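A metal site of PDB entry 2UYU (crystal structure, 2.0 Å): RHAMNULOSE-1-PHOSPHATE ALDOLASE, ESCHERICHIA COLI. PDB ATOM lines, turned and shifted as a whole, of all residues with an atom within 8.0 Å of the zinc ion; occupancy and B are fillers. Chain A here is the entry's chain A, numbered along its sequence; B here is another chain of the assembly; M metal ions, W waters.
Glu 171 of chain B touches the zinc ion (OE2 to ZN, 2.9 Å). Within 4 Å of the zinc ion: His 141, His 143, His 212 and Glu 171 of chain B. The nearest printed residue that does not touch the zinc ion is Gly 31 (4.5 Å).
The zinc ion is bound by a ring nitrogen (NE2) of His 212 (2.0 Å), a ring nitrogen (NE2) of His 141 (2.1 Å), a ring nitrogen (NE2) of His 143 (2.2 Å) and water W1 (2.6 Å).
The backbone carbonyl oxygen (O) of Val 214 is in hydrogen-bond range of a ring nitrogen (ND1) of His 141, 3.0 Å away. The backbone NH of His 141 lies within hydrogen-bond range of the backbone carbonyl oxygen of Asn 32 (2.8 Å). O of Trp 25 lies within hydrogen-bond range of N of His 143, 2.9 Å away. The side-chain carboxylate of Glu 171 of chain B lies close to a ring nitrogen (NE2) of His 143 (3.2 Å). NH2 of Arg 28 lies within salt-bridge range of OE2 of Glu 171 of chain B, 3.97 Å away.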
ATOM      1  N   TRP A  25     -15.833   7.850   0.454  1.00  0.00           N
ATOM      2  CA  TRP A  25     -17.232   8.178   0.671  1.00  0.00           C
ATOM      3  C   TRP A  25     -17.479   9.649   0.940  1.00  0.00           C
ATOM      4  O   TRP A  25     -18.645  10.078   1.043  1.00  0.00           O
ATOM      5  CB  TRP A  25     -17.821   7.435   1.871  1.00  0.00           C
ATOM      6  CG  TRP A  25     -17.779   5.929   1.803  1.00  0.00           C
ATOM      7  CD1 TRP A  25     -17.612   5.181   0.715  1.00  0.00           C
ATOM      8  CD2 TRP A  25     -17.947   5.026   2.916  1.00  0.00           C
ATOM      9  NE1 TRP A  25     -17.615   3.830   1.060  1.00  0.00           N
ATOM     10  CE2 TRP A  25     -17.825   3.726   2.413  1.00  0.00           C
ATOM     11  CE3 TRP A  25     -18.096   5.204   4.297  1.00  0.00           C
ATOM     12  CZ2 TRP A  25     -17.916   2.594   3.237  1.00  0.00           C
ATOM     13  CZ3 TRP A  25     -18.233   4.106   5.107  1.00  0.00           C
ATOM     14  CH2 TRP A  25     -18.109   2.816   4.583  1.00  0.00           C
ATOM     15  N   ASP A  26     -16.441  10.471   1.078  1.00  0.00           N
ATOM     16  CA  ASP A  26     -16.717  11.856   1.542  1.00  0.00           C
ATOM     17  C   ASP A  26     -15.793  12.845   0.878  1.00  0.00           C
ATOM     18  O   ASP A  26     -14.969  13.434   1.535  1.00  0.00           O
ATOM     19  CB  ASP A  26     -16.619  11.983   3.063  1.00  0.00           C
ATOM     20  CG  ASP A  26     -17.685  11.151   3.786  1.00  0.00           C
ATOM     21  OD1 ASP A  26     -17.437   9.957   4.022  1.00  0.00           O
ATOM     22  OD2 ASP A  26     -18.823  11.688   4.082  1.00  0.00           O
ATOM     23  N   GLU A  27     -15.977  13.008  -0.425  1.00  0.00           N
ATOM     24  CA  GLU A  27     -15.396  14.095  -1.250  1.00  0.00           C
ATOM     25  C   GLU A  27     -15.682  15.480  -0.586  1.00  0.00           C
ATOM     26  O   GLU A  27     -16.720  15.659   0.055  1.00  0.00           O
ATOM     27  CB  GLU A  27     -15.982  14.025  -2.723  1.00  0.00           C
ATOM     28  CG  GLU A  27     -17.563  14.444  -3.004  1.00  0.00           C
ATOM     29  CD  GLU A  27     -18.617  13.411  -2.540  1.00  0.00           C
ATOM     30  OE1 GLU A  27     -19.911  13.643  -2.633  1.00  0.00           O
ATOM     31  OE2 GLU A  27     -18.122  12.320  -2.088  1.00  0.00           O
ATOM     32  N   ARG A  28     -14.758  16.442  -0.721  1.00  0.00           N
ATOM     33  CA  ARG A  28     -15.065  17.819  -0.350  1.00  0.00           C
ATOM     34  C   ARG A  28     -15.697  17.814   1.059  1.00  0.00           C
ATOM     35  O   ARG A  28     -15.179  17.171   1.984  1.00  0.00           O
ATOM     36  CB  ARG A  28     -16.053  18.378  -1.406  1.00  0.00           C
ATOM     37  CG  ARG A  28     -15.946  19.922  -1.751  1.00  0.00           C
ATOM     38  CD  ARG A  28     -17.187  20.382  -2.594  1.00  0.00           C
ATOM     39  NE  ARG A  28     -18.456  20.042  -1.881  1.00  0.00           N
ATOM     40  CZ  ARG A  28     -19.244  18.975  -2.107  1.00  0.00           C
ATOM     41  NH1 ARG A  28     -18.979  18.079  -3.084  1.00  0.00           N
ATOM     42  NH2 ARG A  28     -20.338  18.806  -1.350  1.00  0.00           N
ATOM     43  N   ASN A  29     -16.784  18.535   1.213  1.00  0.00           N
ATOM     44  CA  ASN A  29     -17.443  18.675   2.465  1.00  0.00           C
ATOM     45  C   ASN A  29     -18.702  17.751   2.512  1.00  0.00           C
ATOM     46  O   ASN A  29     -19.654  18.010   3.294  1.00  0.00           O
ATOM     47  CB  ASN A  29     -17.821  20.155   2.650  1.00  0.00           C
ATOM     48  CG  ASN A  29     -19.022  20.552   1.851  1.00  0.00           C
ATOM     49  OD1 ASN A  29     -19.122  20.204   0.694  1.00  0.00           O
ATOM     50  ND2 ASN A  29     -20.004  21.261   2.481  1.00  0.00           N
ATOM     51  N   GLY A  30     -18.667  16.654   1.740  1.00  0.00           N
ATOM     52  CA  GLY A  30     -19.811  15.786   1.655  1.00  0.00           C
ATOM     53  C   GLY A  30     -19.876  14.756   2.759  1.00  0.00           C
ATOM     54  O   GLY A  30     -19.083  13.794   2.758  1.00  0.00           O
ATOM     55  N   GLY A  31     -20.792  14.882   3.687  1.00  0.00           N
ATOM     56  CA  GLY A  31     -20.813  13.992   4.822  1.00  0.00           C
ATOM     57  C   GLY A  31     -21.038  14.821   6.078  1.00  0.00           C
ATOM     58  O   GLY A  31     -20.666  16.001   6.076  1.00  0.00           O
ATOM     59  N   ASN A  32     -21.622  14.218   7.137  1.00  0.00           N
ATOM     60  CA  ASN A  32     -21.720  14.844   8.421  1.00  0.00           C
ATOM     61  C   ASN A  32     -21.769  13.773   9.447  1.00  0.00           C
ATOM     62  O   ASN A  32     -22.210  12.688   9.099  1.00  0.00           O
ATOM     63  CB  ASN A  32     -23.073  15.580   8.560  1.00  0.00           C
ATOM     64  CG  ASN A  32     -23.354  16.494   7.411  1.00  0.00           C
ATOM     65  OD1 ASN A  32     -24.022  16.115   6.457  1.00  0.00           O
ATOM     66  ND2 ASN A  32     -22.846  17.715   7.483  1.00  0.00           N
ATOM     67  N   GLU A 117     -26.406  21.673   9.810  1.00  0.00           N
ATOM     68  CA  GLU A 117     -27.122  20.433   9.619  1.00  0.00           C
ATOM     69  C   GLU A 117     -27.516  19.800  10.926  1.00  0.00           C
ATOM     70  O   GLU A 117     -27.974  18.673  10.952  1.00  0.00           O
ATOM     71  CB  GLU A 117     -26.279  19.464   8.785  1.00  0.00           C
ATOM     72  CG  GLU A 117     -26.075  19.973   7.346  1.00  0.00           C
ATOM     73  CD  GLU A 117     -27.399  20.095   6.610  1.00  0.00           C
ATOM     74  OE1 GLU A 117     -28.105  19.075   6.379  1.00  0.00           O
ATOM     75  OE2 GLU A 117     -27.749  21.226   6.254  1.00  0.00           O
ATOM     76  N   HIS A 141     -23.969  10.725   8.038  1.00  0.00           N
ATOM     77  CA  HIS A 141     -24.366  10.839   6.647  1.00  0.00           C
ATOM     78  C   HIS A 141     -23.068  10.757   5.858  1.00  0.00           C
ATOM     79  O   HIS A 141     -22.084  11.432   6.223  1.00  0.00           O
ATOM     80  CB  HIS A 141     -25.003  12.225   6.377  1.00  0.00           C
ATOM     81  CG  HIS A 141     -25.144  12.572   4.909  1.00  0.00           C
ATOM     82  ND1 HIS A 141     -25.891  11.810   4.036  1.00  0.00           N
ATOM     83  CD2 HIS A 141     -24.653  13.601   4.170  1.00  0.00           C
ATOM     84  CE1 HIS A 141     -25.839  12.351   2.822  1.00  0.00           C
ATOM     85  NE2 HIS A 141     -25.119  13.459   2.884  1.00  0.00           N
ATOM     86  N   CYS A 142     -23.006   9.905   4.830  1.00  0.00           N
ATOM     87  CA  CYS A 142     -21.873   9.928   3.920  1.00  0.00           C
ATOM     88  C   CYS A 142     -22.359   9.584   2.526  1.00  0.00           C
ATOM     89  O   CYS A 142     -23.526   9.172   2.362  1.00  0.00           O
ATOM     90  CB  CYS A 142     -20.746   8.946   4.342  1.00  0.00           C
ATOM     91  SG  CYS A 142     -21.357   7.338   4.345  1.00  0.00           S
ATOM     92  N   HIS A 143     -21.477   9.721   1.523  1.00  0.00           N
ATOM     93  CA  HIS A 143     -21.842   9.452   0.146  1.00  0.00           C
ATOM     94  C   HIS A 143     -21.245   8.105  -0.275  1.00  0.00           C
ATOM     95  O   HIS A 143     -20.300   8.036  -1.059  1.00  0.00           O
ATOM     96  CB  HIS A 143     -21.301  10.572  -0.752  1.00  0.00           C
ATOM     97  CG  HIS A 143     -21.897  11.940  -0.422  1.00  0.00           C
ATOM     98  ND1 HIS A 143     -21.503  13.103  -1.078  1.00  0.00           N
ATOM     99  CD2 HIS A 143     -22.909  12.293   0.415  1.00  0.00           C
ATOM    100  CE1 HIS A 143     -22.241  14.123  -0.612  1.00  0.00           C
ATOM    101  NE2 HIS A 143     -23.078  13.652   0.307  1.00  0.00           N
ATOM    102  N   ILE A 148     -25.018   4.697  -3.658  1.00  0.00           N
ATOM    103  CA  ILE A 148     -25.439   5.741  -4.632  1.00  0.00           C
ATOM    104  C   ILE A 148     -25.675   5.132  -6.023  1.00  0.00           C
ATOM    105  O   ILE A 148     -26.738   5.352  -6.649  1.00  0.00           O
ATOM    106  CB  ILE A 148     -24.395   6.904  -4.715  1.00  0.00           C
ATOM    107  CG1 ILE A 148     -24.182   7.518  -3.319  1.00  0.00           C
ATOM    108  CG2 ILE A 148     -24.859   7.961  -5.753  1.00  0.00           C
ATOM    109  CD1 ILE A 148     -23.018   8.509  -3.286  1.00  0.00           C
ATOM    110  N   PRO A 188     -31.626  18.849  -0.647  1.00  0.00           N
ATOM    111  CA  PRO A 188     -30.895  18.731   0.627  1.00  0.00           C
ATOM    112  C   PRO A 188     -30.933  19.985   1.462  1.00  0.00           C
ATOM    113  O   PRO A 188     -30.998  21.080   0.920  1.00  0.00           O
ATOM    114  CB  PRO A 188     -29.446  18.534   0.180  1.00  0.00           C
ATOM    115  CG  PRO A 188     -29.510  18.113  -1.185  1.00  0.00           C
ATOM    116  CD  PRO A 188     -30.699  18.746  -1.799  1.00  0.00           C
ATOM    117  N   TRP A 209     -30.874   8.101   0.427  1.00  0.00           N
ATOM    118  CA  TRP A 209     -31.212   9.249  -0.398  1.00  0.00           C
ATOM    119  C   TRP A 209     -30.690   8.995  -1.831  1.00  0.00           C
ATOM    120  O   TRP A 209     -29.482   8.974  -2.063  1.00  0.00           O
ATOM    121  CB  TRP A 209     -30.523  10.526   0.115  1.00  0.00           C
ATOM    122  CG  TRP A 209     -30.984  11.030   1.479  1.00  0.00           C
ATOM    123  CD1 TRP A 209     -32.083  10.601   2.207  1.00  0.00           C
ATOM    124  CD2 TRP A 209     -30.354  12.054   2.265  1.00  0.00           C
ATOM    125  NE1 TRP A 209     -32.161  11.323   3.395  1.00  0.00           N
ATOM    126  CE2 TRP A 209     -31.120  12.205   3.453  1.00  0.00           C
ATOM    127  CE3 TRP A 209     -29.210  12.856   2.077  1.00  0.00           C
ATOM    128  CZ2 TRP A 209     -30.787  13.136   4.444  1.00  0.00           C
ATOM    129  CZ3 TRP A 209     -28.889  13.791   3.063  1.00  0.00           C
ATOM    130  CH2 TRP A 209     -29.677  13.914   4.238  1.00  0.00           C
ATOM    131  N   HIS A 212     -27.667  10.568  -4.060  1.00  0.00           N
ATOM    132  CA  HIS A 212     -27.025  11.413  -3.064  1.00  0.00           C
ATOM    133  C   HIS A 212     -26.230  10.647  -2.037  1.00  0.00           C
ATOM    134  O   HIS A 212     -25.049  10.941  -1.824  1.00  0.00           O
ATOM    135  CB  HIS A 212     -28.061  12.313  -2.327  1.00  0.00           C
ATOM    136  CG  HIS A 212     -27.434  13.229  -1.332  1.00  0.00           C
ATOM    137  ND1 HIS A 212     -28.037  14.400  -0.904  1.00  0.00           N
ATOM    138  CD2 HIS A 212     -26.257  13.145  -0.679  1.00  0.00           C
ATOM    139  CE1 HIS A 212     -27.245  15.001  -0.019  1.00  0.00           C
ATOM    140  NE2 HIS A 212     -26.151  14.259   0.130  1.00  0.00           N
ATOM    141  N   GLY A 213     -26.881   9.735  -1.291  1.00  0.00           N
ATOM    142  CA  GLY A 213     -26.102   9.104  -0.250  1.00  0.00           C
ATOM    143  C   GLY A 213     -26.944   8.365   0.807  1.00  0.00           C
ATOM    144  O   GLY A 213     -28.060   7.990   0.557  1.00  0.00           O
ATOM    145  N   VAL A 214     -26.368   8.156   1.989  1.00  0.00           N
ATOM    146  CA  VAL A 214     -27.022   7.307   2.972  1.00  0.00           C
ATOM    147  C   VAL A 214     -26.993   8.021   4.292  1.00  0.00           C
ATOM    148  O   VAL A 214     -26.148   8.904   4.514  1.00  0.00           O
ATOM    149  CB  VAL A 214     -26.288   5.956   3.011  1.00  0.00           C
ATOM    150  CG1 VAL A 214     -24.897   6.128   3.614  1.00  0.00           C
ATOM    151  CG2 VAL A 214     -27.082   4.974   3.823  1.00  0.00           C
ATOM    152  N   PHE A 215     -27.886   7.661   5.187  1.00  0.00           N
ATOM    153  CA  PHE A 215     -27.984   8.297   6.481  1.00  0.00           C
ATOM    154  C   PHE A 215     -28.189   7.146   7.491  1.00  0.00           C
ATOM    155  O   PHE A 215     -29.155   6.402   7.356  1.00  0.00           O
ATOM    156  CB  PHE A 215     -29.221   9.169   6.427  1.00  0.00           C
ATOM    157  CG  PHE A 215     -29.226  10.307   7.389  1.00  0.00           C
ATOM    158  CD1 PHE A 215     -28.675  11.525   7.044  1.00  0.00           C
ATOM    159  CD2 PHE A 215     -29.903  10.182   8.597  1.00  0.00           C
ATOM    160  CE1 PHE A 215     -28.726  12.597   7.921  1.00  0.00           C
ATOM    161  CE2 PHE A 215     -30.004  11.243   9.493  1.00  0.00           C
ATOM    162  CZ  PHE A 215     -29.391  12.477   9.144  1.00  0.00           C
ATOM    163  N   THR B 170     -25.851  14.582  -6.304  1.00  0.00           N
ATOM    164  CA  THR B 170     -26.746  15.717  -6.040  1.00  0.00           C
ATOM    165  C   THR B 170     -26.060  17.052  -5.916  1.00  0.00           C
ATOM    166  O   THR B 170     -26.535  18.055  -6.459  1.00  0.00           O
ATOM    167  CB  THR B 170     -27.611  15.427  -4.813  1.00  0.00           C
ATOM    168  OG1 THR B 170     -28.518  14.382  -5.165  1.00  0.00           O
ATOM    169  CG2 THR B 170     -28.420  16.663  -4.386  1.00  0.00           C
ATOM    170  N   GLU B 171     -24.940  17.092  -5.209  1.00  0.00           N
ATOM    171  CA  GLU B 171     -24.339  18.352  -4.903  1.00  0.00           C
ATOM    172  C   GLU B 171     -23.510  18.978  -6.068  1.00  0.00           C
ATOM    173  O   GLU B 171     -23.159  20.186  -6.008  1.00  0.00           O
ATOM    174  CB  GLU B 171     -23.630  18.303  -3.527  1.00  0.00           C
ATOM    175  CG  GLU B 171     -24.679  18.090  -2.353  1.00  0.00           C
ATOM    176  CD  GLU B 171     -24.103  17.760  -0.959  1.00  0.00           C
ATOM    177  OE1 GLU B 171     -24.248  18.604  -0.077  1.00  0.00           O
ATOM    178  OE2 GLU B 171     -23.613  16.662  -0.692  1.00  0.00           O
HETATM  179 ZN    ZN M   1     -24.611  14.800   1.310  1.00  0.00          ZN
HETATM  180  O   HOH W   1     -26.077  16.729   2.152  1.00  0.00           O
